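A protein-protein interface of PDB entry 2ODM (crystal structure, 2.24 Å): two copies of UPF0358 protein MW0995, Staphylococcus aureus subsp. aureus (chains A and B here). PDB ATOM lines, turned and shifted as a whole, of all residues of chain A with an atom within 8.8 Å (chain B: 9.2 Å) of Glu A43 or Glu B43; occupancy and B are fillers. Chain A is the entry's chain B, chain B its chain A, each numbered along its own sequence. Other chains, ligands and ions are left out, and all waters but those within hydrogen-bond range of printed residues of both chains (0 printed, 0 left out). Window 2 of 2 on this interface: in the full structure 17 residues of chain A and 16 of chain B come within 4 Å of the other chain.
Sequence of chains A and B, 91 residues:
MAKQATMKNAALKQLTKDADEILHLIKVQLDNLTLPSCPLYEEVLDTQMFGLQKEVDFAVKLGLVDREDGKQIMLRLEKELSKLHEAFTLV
OE1 of Glu A43 sits close to OE1 of Glu B43 (3.1 Å).
O of Glu B43 is in hydrogen-bond range of OG1 of Thr B47, at 3.2 Å.
The backbone carbonyl oxygen (O) of Glu A43 sits at hydrogen-bond distance from the side-chain hydroxyl (OG1) of Thr A47.
O of Thr A47 touches CE2 of Phe B50, at 3.6 Å.
CZ of Phe B50 touches NE2 of Gln A48, at 3.8 Å.
Phe A50 touches Thr B47.
Gln B48 touches Phe A50.
Glu A43 touches just one residue of chain B: Glu B43 (3.1 Å).
No residue of chain B comes within 4 Å of Val A44.
Of the printed residues of chain B, Thr A47 touches Phe B50 (3.6 Å).
Of the printed residues of chain B, Gln A48 touches Phe B50.
Of the printed residues of chain B, Phe A50 touches Thr B47 (3.5 Å) and Gln B48 (3.7 Å).
Of the printed residues of chain A, Thr B47 touches Phe A50 (3.5 Å).
Of the printed residues of chain A, Phe B50 touches Thr A47 and Gln A48.
The nearest residue of chain B that does not touch Glu A43 is Thr B47 (7.0 Å).
The nearest residue of chain A that does not touch Glu B43 is Thr A47 (7.2 Å).
Of the 18 printed residues of chain B, 4 touch a printed residue of chain A.
Hydrophobic or aromatic side chains of chain B that line the printed part of chain A: Phe B50.
Hydrophobic or aromatic side chains of chain A that line the printed part of chain B: Phe A50.
Along chain A the printed residues that touch a printed residue of chain B span positions 43 to 50.
Glu A43 touches its own counterpart, Glu B43.
Thr A47 touches Phe B50, and with the chains exchanged Phe A50 touches Thr B47.
Gln A48 touches Phe B50, and with the chains exchanged Phe A50 touches Gln B48.
16 positions are printed for both chains.
Of the 5 pairs that touch across the chains among the printed residues, 5 have their exchanged pair printed and touching as well.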
ATOM      1  N   LEU A  25     -26.868   0.306   7.873  1.00  0.00           N
ATOM      2  CA  LEU A  25     -27.169   0.261   6.436  1.00  0.00           C
ATOM      3  C   LEU A  25     -28.587  -0.250   6.162  1.00  0.00           C
ATOM      4  O   LEU A  25     -29.281   0.279   5.302  1.00  0.00           O
ATOM      5  CB  LEU A  25     -26.166  -0.654   5.728  1.00  0.00           C
ATOM      6  CG  LEU A  25     -25.562  -0.276   4.382  1.00  0.00           C
ATOM      7  CD1 LEU A  25     -24.442   0.738   4.572  1.00  0.00           C
ATOM      8  CD2 LEU A  25     -25.012  -1.520   3.717  1.00  0.00           C
ATOM      9  N   CYS A  38     -31.054  -1.109  -7.723  1.00  0.00           N
ATOM     10  CA  CYS A  38     -31.833  -1.519  -6.557  1.00  0.00           C
ATOM     11  C   CYS A  38     -31.730  -3.023  -6.257  1.00  0.00           C
ATOM     12  O   CYS A  38     -31.557  -3.396  -5.092  1.00  0.00           O
ATOM     13  CB  CYS A  38     -33.297  -1.081  -6.685  1.00  0.00           C
ATOM     14  SG  CYS A  38     -34.271  -1.335  -5.183  1.00  0.00           S
ATOM     15  N   PRO A  39     -31.850  -3.892  -7.291  1.00  0.00           N
ATOM     16  CA  PRO A  39     -31.521  -5.307  -7.066  1.00  0.00           C
ATOM     17  C   PRO A  39     -30.048  -5.508  -6.697  1.00  0.00           C
ATOM     18  O   PRO A  39     -29.686  -6.545  -6.130  1.00  0.00           O
ATOM     19  CB  PRO A  39     -31.831  -5.964  -8.419  1.00  0.00           C
ATOM     20  CG  PRO A  39     -32.767  -5.025  -9.099  1.00  0.00           C
ATOM     21  CD  PRO A  39     -32.315  -3.664  -8.674  1.00  0.00           C
ATOM     22  N   LEU A  40     -29.219  -4.519  -7.031  1.00  0.00           N
ATOM     23  CA  LEU A  40     -27.823  -4.468  -6.607  1.00  0.00           C
ATOM     24  C   LEU A  40     -27.747  -4.239  -5.096  1.00  0.00           C
ATOM     25  O   LEU A  40     -26.990  -4.921  -4.402  1.00  0.00           O
ATOM     26  CB  LEU A  40     -27.073  -3.366  -7.376  1.00  0.00           C
ATOM     27  CG  LEU A  40     -25.574  -3.112  -7.149  1.00  0.00           C
ATOM     28  CD1 LEU A  40     -24.892  -2.715  -8.454  1.00  0.00           C
ATOM     29  CD2 LEU A  40     -25.337  -2.046  -6.075  1.00  0.00           C
ATOM     30  N   TYR A  41     -28.545  -3.295  -4.592  1.00  0.00           N
ATOM     31  CA  TYR A  41     -28.581  -2.983  -3.161  1.00  0.00           C
ATOM     32  C   TYR A  41     -29.450  -3.978  -2.377  1.00  0.00           C
ATOM     33  O   TYR A  41     -30.326  -3.593  -1.597  1.00  0.00           O
ATOM     34  CB  TYR A  41     -29.043  -1.541  -2.917  1.00  0.00           C
ATOM     35  CG  TYR A  41     -28.335  -0.867  -1.761  1.00  0.00           C
ATOM     36  CD1 TYR A  41     -27.499   0.230  -1.975  1.00  0.00           C
ATOM     37  CD2 TYR A  41     -28.486  -1.334  -0.454  1.00  0.00           C
ATOM     38  CE1 TYR A  41     -26.838   0.850  -0.912  1.00  0.00           C
ATOM     39  CE2 TYR A  41     -27.833  -0.725   0.612  1.00  0.00           C
ATOM     40  CZ  TYR A  41     -27.012   0.365   0.379  1.00  0.00           C
ATOM     41  OH  TYR A  41     -26.370   0.962   1.441  1.00  0.00           O
ATOM     42  N   GLU A  42     -29.198  -5.259  -2.617  1.00  0.00           N
ATOM     43  CA  GLU A  42     -29.825  -6.359  -1.901  1.00  0.00           C
ATOM     44  C   GLU A  42     -28.807  -7.488  -1.873  1.00  0.00           C
ATOM     45  O   GLU A  42     -28.687  -8.201  -0.879  1.00  0.00           O
ATOM     46  CB  GLU A  42     -31.102  -6.825  -2.598  1.00  0.00           C
ATOM     47  CG  GLU A  42     -31.985  -7.706  -1.729  1.00  0.00           C
ATOM     48  CD  GLU A  42     -32.571  -8.878  -2.492  1.00  0.00           C
ATOM     49  OE1 GLU A  42     -31.873  -9.908  -2.621  1.00  0.00           O
ATOM     50  OE2 GLU A  42     -33.730  -8.778  -2.951  1.00  0.00           O
ATOM     51  N   GLU A  43     -28.089  -7.644  -2.986  1.00  0.00           N
ATOM     52  CA  GLU A  43     -26.931  -8.526  -3.047  1.00  0.00           C
ATOM     53  C   GLU A  43     -25.804  -7.949  -2.198  1.00  0.00           C
ATOM     54  O   GLU A  43     -25.101  -8.690  -1.519  1.00  0.00           O
ATOM     55  CB  GLU A  43     -26.464  -8.721  -4.485  1.00  0.00           C
ATOM     56  CG  GLU A  43     -27.207  -9.812  -5.230  1.00  0.00           C
ATOM     57  CD  GLU A  43     -26.403 -10.392  -6.383  1.00  0.00           C
ATOM     58  OE1 GLU A  43     -26.335 -11.636  -6.484  1.00  0.00           O
ATOM     59  OE2 GLU A  43     -25.835  -9.611  -7.181  1.00  0.00           O
ATOM     60  N   VAL A  44     -25.653  -6.625  -2.237  1.00  0.00           N
ATOM     61  CA  VAL A  44     -24.699  -5.921  -1.391  1.00  0.00           C
ATOM     62  C   VAL A  44     -24.922  -6.262   0.086  1.00  0.00           C
ATOM     63  O   VAL A  44     -23.969  -6.554   0.803  1.00  0.00           O
ATOM     64  CB  VAL A  44     -24.759  -4.392  -1.614  1.00  0.00           C
ATOM     65  CG1 VAL A  44     -24.025  -3.655  -0.510  1.00  0.00           C
ATOM     66  CG2 VAL A  44     -24.165  -4.038  -2.962  1.00  0.00           C
ATOM     67  N   LEU A  45     -26.180  -6.245   0.524  1.00  0.00           N
ATOM     68  CA  LEU A  45     -26.529  -6.590   1.905  1.00  0.00           C
ATOM     69  C   LEU A  45     -26.300  -8.073   2.210  1.00  0.00           C
ATOM     70  O   LEU A  45     -25.810  -8.418   3.286  1.00  0.00           O
ATOM     71  CB  LEU A  45     -27.962  -6.141   2.240  1.00  0.00           C
ATOM     72  CG  LEU A  45     -28.106  -4.616   2.452  1.00  0.00           C
ATOM     73  CD1 LEU A  45     -29.548  -4.167   2.340  1.00  0.00           C
ATOM     74  CD2 LEU A  45     -27.515  -4.158   3.786  1.00  0.00           C
ATOM     75  N   ASP A  46     -26.620  -8.933   1.246  1.00  0.00           N
ATOM     76  CA  ASP A  46     -26.306 -10.367   1.324  1.00  0.00           C
ATOM     77  C   ASP A  46     -24.805 -10.644   1.461  1.00  0.00           C
ATOM     78  O   ASP A  46     -24.396 -11.477   2.261  1.00  0.00           O
ATOM     79  CB  ASP A  46     -26.874 -11.115   0.107  1.00  0.00           C
ATOM     80  CG  ASP A  46     -28.402 -11.213   0.131  1.00  0.00           C
ATOM     81  OD1 ASP A  46     -28.994 -11.442  -0.945  1.00  0.00           O
ATOM     82  OD2 ASP A  46     -29.015 -11.056   1.213  1.00  0.00           O
ATOM     83  N   THR A  47     -23.993  -9.934   0.681  1.00  0.00           N
ATOM     84  CA  THR A  47     -22.539 -10.033   0.779  1.00  0.00           C
ATOM     85  C   THR A  47     -22.044  -9.560   2.151  1.00  0.00           C
ATOM     86  O   THR A  47     -21.187 -10.190   2.767  1.00  0.00           O
ATOM     87  CB  THR A  47     -21.845  -9.243  -0.371  1.00  0.00           C
ATOM     88  OG1 THR A  47     -22.350  -9.702  -1.627  1.00  0.00           O
ATOM     89  CG2 THR A  47     -20.342  -9.450  -0.359  1.00  0.00           C
ATOM     90  N   GLN A  48     -22.597  -8.448   2.621  1.00  0.00           N
ATOM     91  CA  GLN A  48     -22.267  -7.896   3.928  1.00  0.00           C
ATOM     92  C   GLN A  48     -22.542  -8.902   5.050  1.00  0.00           C
ATOM     93  O   GLN A  48     -21.724  -9.078   5.959  1.00  0.00           O
ATOM     94  CB  GLN A  48     -23.108  -6.638   4.157  1.00  0.00           C
ATOM     95  CG  GLN A  48     -22.337  -5.432   4.621  1.00  0.00           C
ATOM     96  CD  GLN A  48     -21.850  -4.587   3.476  1.00  0.00           C
ATOM     97  OE1 GLN A  48     -22.168  -3.407   3.397  1.00  0.00           O
ATOM     98  NE2 GLN A  48     -21.080  -5.184   2.576  1.00  0.00           N
ATOM     99  N   MET A  49     -23.719  -9.524   4.990  1.00  0.00           N
ATOM    100  CA  MET A  49     -24.149 -10.538   5.955  1.00  0.00           C
ATOM    101  C   MET A  49     -23.230 -11.767   5.939  1.00  0.00           C
ATOM    102  O   MET A  49     -22.866 -12.284   6.993  1.00  0.00           O
ATOM    103  CB  MET A  49     -25.597 -10.962   5.649  1.00  0.00           C
ATOM    104  CG  MET A  49     -26.636  -9.849   5.876  1.00  0.00           C
ATOM    105  SD  MET A  49     -26.755  -9.342   7.746  1.00  0.00           S
ATOM    106  CE  MET A  49     -27.826 -10.888   8.385  1.00  0.00           C
ATOM    107  N   PHE A  50     -22.881 -12.224   4.735  1.00  0.00           N
ATOM    108  CA  PHE A  50     -21.919 -13.309   4.530  1.00  0.00           C
ATOM    109  C   PHE A  50     -20.570 -13.003   5.173  1.00  0.00           C
ATOM    110  O   PHE A  50     -19.988 -13.858   5.840  1.00  0.00           O
ATOM    111  CB  PHE A  50     -21.747 -13.611   3.025  1.00  0.00           C
ATOM    112  CG  PHE A  50     -20.831 -14.788   2.733  1.00  0.00           C
ATOM    113  CD1 PHE A  50     -21.328 -16.088   2.709  1.00  0.00           C
ATOM    114  CD2 PHE A  50     -19.471 -14.590   2.482  1.00  0.00           C
ATOM    115  CE1 PHE A  50     -20.479 -17.177   2.442  1.00  0.00           C
ATOM    116  CE2 PHE A  50     -18.618 -15.667   2.220  1.00  0.00           C
ATOM    117  CZ  PHE A  50     -19.127 -16.963   2.196  1.00  0.00           C
ATOM    118  N   GLY A  51     -20.082 -11.781   4.972  1.00  0.00           N
ATOM    119  CA  GLY A  51     -18.833 -11.337   5.584  1.00  0.00           C
ATOM    120  C   GLY A  51     -18.873 -11.318   7.096  1.00  0.00           C
ATOM    121  O   GLY A  51     -17.920 -11.738   7.764  1.00  0.00           O
ATOM    122  N   LEU A  81     -33.184  -7.452   8.443  1.00  0.00           N
ATOM    123  CA  LEU A  81     -33.107  -7.760   7.014  1.00  0.00           C
ATOM    124  C   LEU A  81     -34.393  -8.419   6.474  1.00  0.00           C
ATOM    125  O   LEU A  81     -34.795  -8.160   5.334  1.00  0.00           O
ATOM    126  CB  LEU A  81     -31.873  -8.623   6.724  1.00  0.00           C
ATOM    127  CG  LEU A  81     -31.430  -8.753   5.266  1.00  0.00           C
ATOM    128  CD1 LEU A  81     -30.674  -7.522   4.810  1.00  0.00           C
ATOM    129  CD2 LEU A  81     -30.593 -10.026   5.059  1.00  0.00           C
ATOM    130  N   HIS A  85     -36.631  -7.120   3.405  1.00  0.00           N
ATOM    131  CA  HIS A  85     -37.058  -7.994   2.314  1.00  0.00           C
ATOM    132  C   HIS A  85     -38.571  -7.951   2.116  1.00  0.00           C
ATOM    133  O   HIS A  85     -39.044  -7.831   0.986  1.00  0.00           O
ATOM    134  CB  HIS A  85     -36.589  -9.433   2.547  1.00  0.00           C
ATOM    135  CG  HIS A  85     -35.111  -9.619   2.385  1.00  0.00           C
ATOM    136  ND1 HIS A  85     -34.369  -8.917   1.460  1.00  0.00           N
ATOM    137  CD2 HIS A  85     -34.242 -10.441   3.018  1.00  0.00           C
ATOM    138  CE1 HIS A  85     -33.105  -9.290   1.537  1.00  0.00           C
ATOM    139  NE2 HIS A  85     -33.001 -10.216   2.473  1.00  0.00           N
ATOM    140  N   PHE A  88     -39.419  -4.653   0.588  1.00  0.00           N
ATOM    141  CA  PHE A  88     -39.091  -4.699  -0.842  1.00  0.00           C
ATOM    142  C   PHE A  88     -40.251  -5.237  -1.686  1.00  0.00           C
ATOM    143  O   PHE A  88     -40.562  -4.678  -2.740  1.00  0.00           O
ATOM    144  CB  PHE A  88     -37.843  -5.555  -1.104  1.00  0.00           C
ATOM    145  CG  PHE A  88     -36.529  -4.852  -0.843  1.00  0.00           C
ATOM    146  CD1 PHE A  88     -35.397  -5.596  -0.507  1.00  0.00           C
ATOM    147  CD2 PHE A  88     -36.411  -3.469  -0.947  1.00  0.00           C
ATOM    148  CE1 PHE A  88     -34.172  -4.975  -0.279  1.00  0.00           C
ATOM    149  CE2 PHE A  88     -35.191  -2.834  -0.715  1.00  0.00           C
ATOM    150  CZ  PHE A  88     -34.070  -3.590  -0.380  1.00  0.00           C
ATOM    151  N   LEU B  25     -10.940 -24.228  -4.379  1.00  0.00           N
ATOM    152  CA  LEU B  25     -11.983 -23.881  -5.344  1.00  0.00           C
ATOM    153  C   LEU B  25     -11.392 -23.243  -6.611  1.00  0.00           C
ATOM    154  O   LEU B  25     -11.803 -23.574  -7.726  1.00  0.00           O
ATOM    155  CB  LEU B  25     -13.043 -22.983  -4.692  1.00  0.00           C
ATOM    156  CG  LEU B  25     -14.310 -22.575  -5.451  1.00  0.00           C
ATOM    157  CD1 LEU B  25     -14.991 -23.759  -6.155  1.00  0.00           C
ATOM    158  CD2 LEU B  25     -15.283 -21.876  -4.501  1.00  0.00           C
ATOM    159  N   GLN B  29     -10.802 -25.085 -10.520  1.00  0.00           N
ATOM    160  CA  GLN B  29     -11.235 -24.384 -11.730  1.00  0.00           C
ATOM    161  C   GLN B  29     -10.125 -24.321 -12.787  1.00  0.00           C
ATOM    162  O   GLN B  29     -10.399 -24.429 -13.981  1.00  0.00           O
ATOM    163  CB  GLN B  29     -11.732 -22.973 -11.400  1.00  0.00           C
ATOM    164  CG  GLN B  29     -13.077 -22.910 -10.686  1.00  0.00           C
ATOM    165  CD  GLN B  29     -14.250 -23.179 -11.610  1.00  0.00           C
ATOM    166  OE1 GLN B  29     -14.536 -24.326 -11.958  1.00  0.00           O
ATOM    167  NE2 GLN B  29     -14.946 -22.118 -12.001  1.00  0.00           N
ATOM    168  N   CYS B  38     -16.913 -20.450 -15.335  1.00  0.00           N
ATOM    169  CA  CYS B  38     -18.052 -20.671 -16.217  1.00  0.00           C
ATOM    170  C   CYS B  38     -19.319 -21.024 -15.434  1.00  0.00           C
ATOM    171  O   CYS B  38     -19.307 -21.957 -14.625  1.00  0.00           O
ATOM    172  CB  CYS B  38     -17.740 -21.770 -17.239  1.00  0.00           C
ATOM    173  SG  CYS B  38     -16.490 -21.318 -18.461  1.00  0.00           S
ATOM    174  N   PRO B  39     -20.413 -20.269 -15.659  1.00  0.00           N
ATOM    175  CA  PRO B  39     -20.458 -19.075 -16.509  1.00  0.00           C
ATOM    176  C   PRO B  39     -19.947 -17.843 -15.759  1.00  0.00           C
ATOM    177  O   PRO B  39     -18.904 -17.290 -16.118  1.00  0.00           O
ATOM    178  CB  PRO B  39     -21.950 -18.934 -16.855  1.00  0.00           C
ATOM    179  CG  PRO B  39     -22.666 -20.061 -16.129  1.00  0.00           C
ATOM    180  CD  PRO B  39     -21.735 -20.568 -15.082  1.00  0.00           C
ATOM    181  N   LEU B  40     -20.681 -17.428 -14.727  1.00  0.00           N
ATOM    182  CA  LEU B  40     -20.226 -16.386 -13.813  1.00  0.00           C
ATOM    183  C   LEU B  40     -19.877 -17.018 -12.463  1.00  0.00           C
ATOM    184  O   LEU B  40     -20.497 -16.727 -11.436  1.00  0.00           O
ATOM    185  CB  LEU B  40     -21.278 -15.272 -13.655  1.00  0.00           C
ATOM    186  CG  LEU B  40     -21.736 -14.377 -14.826  1.00  0.00           C
ATOM    187  CD1 LEU B  40     -20.591 -13.926 -15.741  1.00  0.00           C
ATOM    188  CD2 LEU B  40     -22.864 -15.022 -15.635  1.00  0.00           C
ATOM    189  N   TYR B  41     -18.882 -17.904 -12.489  1.00  0.00           N
ATOM    190  CA  TYR B  41     -18.342 -18.525 -11.282  1.00  0.00           C
ATOM    191  C   TYR B  41     -17.446 -17.516 -10.566  1.00  0.00           C
ATOM    192  O   TYR B  41     -17.028 -17.735  -9.426  1.00  0.00           O
ATOM    193  CB  TYR B  41     -17.535 -19.768 -11.656  1.00  0.00           C
ATOM    194  CG  TYR B  41     -17.666 -20.923 -10.689  1.00  0.00           C
ATOM    195  CD1 TYR B  41     -16.887 -20.988  -9.532  1.00  0.00           C
ATOM    196  CD2 TYR B  41     -18.560 -21.966 -10.940  1.00  0.00           C
ATOM    197  CE1 TYR B  41     -17.001 -22.056  -8.646  1.00  0.00           C
ATOM    198  CE2 TYR B  41     -18.682 -23.040 -10.061  1.00  0.00           C
ATOM    199  CZ  TYR B  41     -17.899 -23.078  -8.917  1.00  0.00           C
ATOM    200  OH  TYR B  41     -18.017 -24.137  -8.046  1.00  0.00           O
ATOM    201  N   GLU B  42     -17.157 -16.419 -11.268  1.00  0.00           N
ATOM    202  CA  GLU B  42     -16.424 -15.272 -10.741  1.00  0.00           C
ATOM    203  C   GLU B  42     -17.191 -14.608  -9.597  1.00  0.00           C
ATOM    204  O   GLU B  42     -16.582 -14.158  -8.626  1.00  0.00           O
ATOM    205  CB  GLU B  42     -16.174 -14.254 -11.863  1.00  0.00           C
ATOM    206  CG  GLU B  42     -15.241 -13.094 -11.494  1.00  0.00           C
ATOM    207  CD  GLU B  42     -15.272 -11.947 -12.502  1.00  0.00           C
ATOM    208  OE1 GLU B  42     -15.856 -12.111 -13.596  1.00  0.00           O
ATOM    209  OE2 GLU B  42     -14.704 -10.876 -12.194  1.00  0.00           O
ATOM    210  N   GLU B  43     -18.521 -14.547  -9.728  1.00  0.00           N
ATOM    211  CA  GLU B  43     -19.399 -13.997  -8.687  1.00  0.00           C
ATOM    212  C   GLU B  43     -19.214 -14.744  -7.376  1.00  0.00           C
ATOM    213  O   GLU B  43     -19.134 -14.128  -6.313  1.00  0.00           O
ATOM    214  CB  GLU B  43     -20.876 -14.064  -9.106  1.00  0.00           C
ATOM    215  CG  GLU B  43     -21.858 -13.586  -8.021  1.00  0.00           C
ATOM    216  CD  GLU B  43     -23.311 -14.003  -8.264  1.00  0.00           C
ATOM    217  OE1 GLU B  43     -24.195 -13.117  -8.219  1.00  0.00           O
ATOM    218  OE2 GLU B  43     -23.577 -15.208  -8.485  1.00  0.00           O
ATOM    219  N   VAL B  44     -19.149 -16.073  -7.473  1.00  0.00           N
ATOM    220  CA  VAL B  44     -19.032 -16.953  -6.317  1.00  0.00           C
ATOM    221  C   VAL B  44     -17.720 -16.718  -5.572  1.00  0.00           C
ATOM    222  O   VAL B  44     -17.709 -16.561  -4.353  1.00  0.00           O
ATOM    223  CB  VAL B  44     -19.155 -18.449  -6.726  1.00  0.00           C
ATOM    224  CG1 VAL B  44     -18.884 -19.369  -5.538  1.00  0.00           C
ATOM    225  CG2 VAL B  44     -20.530 -18.733  -7.314  1.00  0.00           C
ATOM    226  N   LEU B  45     -16.625 -16.681  -6.323  1.00  0.00           N
ATOM    227  CA  LEU B  45     -15.297 -16.473  -5.766  1.00  0.00           C
ATOM    228  C   LEU B  45     -15.115 -15.090  -5.146  1.00  0.00           C
ATOM    229  O   LEU B  45     -14.446 -14.958  -4.124  1.00  0.00           O
ATOM    230  CB  LEU B  45     -14.225 -16.741  -6.828  1.00  0.00           C
ATOM    231  CG  LEU B  45     -14.084 -18.211  -7.241  1.00  0.00           C
ATOM    232  CD1 LEU B  45     -13.266 -18.332  -8.508  1.00  0.00           C
ATOM    233  CD2 LEU B  45     -13.471 -19.032  -6.110  1.00  0.00           C
ATOM    234  N   ASP B  46     -15.704 -14.072  -5.769  1.00  0.00           N
ATOM    235  CA  ASP B  46     -15.680 -12.713  -5.233  1.00  0.00           C
ATOM    236  C   ASP B  46     -16.299 -12.624  -3.833  1.00  0.00           C
ATOM    237  O   ASP B  46     -15.769 -11.949  -2.951  1.00  0.00           O
ATOM    238  CB  ASP B  46     -16.379 -11.746  -6.195  1.00  0.00           C
ATOM    239  CG  ASP B  46     -15.521 -11.391  -7.402  1.00  0.00           C
ATOM    240  OD1 ASP B  46     -14.334 -11.792  -7.454  1.00  0.00           O
ATOM    241  OD2 ASP B  46     -16.039 -10.706  -8.308  1.00  0.00           O
ATOM    242  N   THR B  47     -17.417 -13.317  -3.639  1.00  0.00           N
ATOM    243  CA  THR B  47     -18.063 -13.412  -2.330  1.00  0.00           C
ATOM    244  C   THR B  47     -17.181 -14.152  -1.310  1.00  0.00           C
ATOM    245  O   THR B  47     -17.048 -13.713  -0.167  1.00  0.00           O
ATOM    246  CB  THR B  47     -19.451 -14.067  -2.465  1.00  0.00           C
ATOM    247  OG1 THR B  47     -20.227 -13.302  -3.392  1.00  0.00           O
ATOM    248  CG2 THR B  47     -20.185 -14.123  -1.126  1.00  0.00           C
ATOM    249  N   GLN B  48     -16.563 -15.253  -1.738  1.00  0.00           N
ATOM    250  CA  GLN B  48     -15.617 -16.005  -0.897  1.00  0.00           C
ATOM    251  C   GLN B  48     -14.397 -15.170  -0.500  1.00  0.00           C
ATOM    252  O   GLN B  48     -13.959 -15.205   0.646  1.00  0.00           O
ATOM    253  CB  GLN B  48     -15.151 -17.269  -1.617  1.00  0.00           C
ATOM    254  CG  GLN B  48     -16.274 -18.148  -2.122  1.00  0.00           C
ATOM    255  CD  GLN B  48     -16.772 -19.098  -1.075  1.00  0.00           C
ATOM    256  OE1 GLN B  48     -17.923 -19.027  -0.648  1.00  0.00           O
ATOM    257  NE2 GLN B  48     -15.900 -19.991  -0.639  1.00  0.00           N
ATOM    258  N   MET B  49     -13.850 -14.429  -1.462  1.00  0.00           N
ATOM    259  CA  MET B  49     -12.722 -13.535  -1.217  1.00  0.00           C
ATOM    260  C   MET B  49     -13.094 -12.410  -0.236  1.00  0.00           C
ATOM    261  O   MET B  49     -12.297 -12.044   0.639  1.00  0.00           O
ATOM    262  CB  MET B  49     -12.214 -12.942  -2.541  1.00  0.00           C
ATOM    263  CG  MET B  49     -11.573 -13.972  -3.470  1.00  0.00           C
ATOM    264  SD  MET B  49      -9.984 -14.723  -2.671  1.00  0.00           S
ATOM    265  CE  MET B  49      -8.700 -13.490  -3.415  1.00  0.00           C
ATOM    266  N   PHE B  50     -14.304 -11.877  -0.389  1.00  0.00           N
ATOM    267  CA  PHE B  50     -14.833 -10.861   0.528  1.00  0.00           C
ATOM    268  C   PHE B  50     -14.934 -11.399   1.955  1.00  0.00           C
ATOM    269  O   PHE B  50     -14.515 -10.727   2.899  1.00  0.00           O
ATOM    270  CB  PHE B  50     -16.203 -10.357   0.033  1.00  0.00           C
ATOM    271  CG  PHE B  50     -16.759  -9.209   0.836  1.00  0.00           C
ATOM    272  CD1 PHE B  50     -16.440  -7.892   0.506  1.00  0.00           C
ATOM    273  CD2 PHE B  50     -17.589  -9.446   1.930  1.00  0.00           C
ATOM    274  CE1 PHE B  50     -16.948  -6.827   1.253  1.00  0.00           C
ATOM    275  CE2 PHE B  50     -18.102  -8.391   2.687  1.00  0.00           C
ATOM    276  CZ  PHE B  50     -17.787  -7.082   2.348  1.00  0.00           C
ATOM    277  N   LEU B  81      -6.119 -16.279  -8.453  1.00  0.00           N
ATOM    278  CA  LEU B  81      -7.407 -15.853  -9.003  1.00  0.00           C
ATOM    279  C   LEU B  81      -7.236 -15.133 -10.340  1.00  0.00           C
ATOM    280  O   LEU B  81      -8.134 -15.161 -11.184  1.00  0.00           O
ATOM    281  CB  LEU B  81      -8.129 -14.933  -8.015  1.00  0.00           C
ATOM    282  CG  LEU B  81      -9.608 -15.145  -7.660  1.00  0.00           C
ATOM    283  CD1 LEU B  81     -10.151 -13.898  -6.971  1.00  0.00           C
ATOM    284  CD2 LEU B  81     -10.479 -15.507  -8.847  1.00  0.00           C
ATOM    285  N   LEU B  84      -7.188 -17.228 -13.493  1.00  0.00           N
ATOM    286  CA  LEU B  84      -8.486 -17.803 -13.823  1.00  0.00           C
ATOM    287  C   LEU B  84      -9.227 -17.010 -14.901  1.00  0.00           C
ATOM    288  O   LEU B  84      -9.978 -17.586 -15.690  1.00  0.00           O
ATOM    289  CB  LEU B  84      -9.340 -17.967 -12.562  1.00  0.00           C
ATOM    290  CG  LEU B  84     -10.533 -18.929 -12.610  1.00  0.00           C
ATOM    291  CD1 LEU B  84     -10.194 -20.239 -13.320  1.00  0.00           C
ATOM    292  CD2 LEU B  84     -11.040 -19.199 -11.209  1.00  0.00           C
ATOM    293  N   HIS B  85      -9.014 -15.696 -14.930  1.00  0.00           N
ATOM    294  CA  HIS B  85      -9.604 -14.839 -15.964  1.00  0.00           C
ATOM    295  C   HIS B  85      -8.641 -13.747 -16.448  1.00  0.00           C
ATOM    296  O   HIS B  85      -8.345 -12.821 -15.693  1.00  0.00           O
ATOM    297  CB  HIS B  85     -10.935 -14.221 -15.499  1.00  0.00           C
ATOM    298  CG  HIS B  85     -10.964 -13.833 -14.052  1.00  0.00           C
ATOM    299  ND1 HIS B  85     -11.919 -14.306 -13.177  1.00  0.00           N
ATOM    300  CD2 HIS B  85     -10.158 -13.024 -13.325  1.00  0.00           C
ATOM    301  CE1 HIS B  85     -11.701 -13.802 -11.975  1.00  0.00           C
ATOM    302  NE2 HIS B  85     -10.637 -13.023 -12.037  1.00  0.00           N
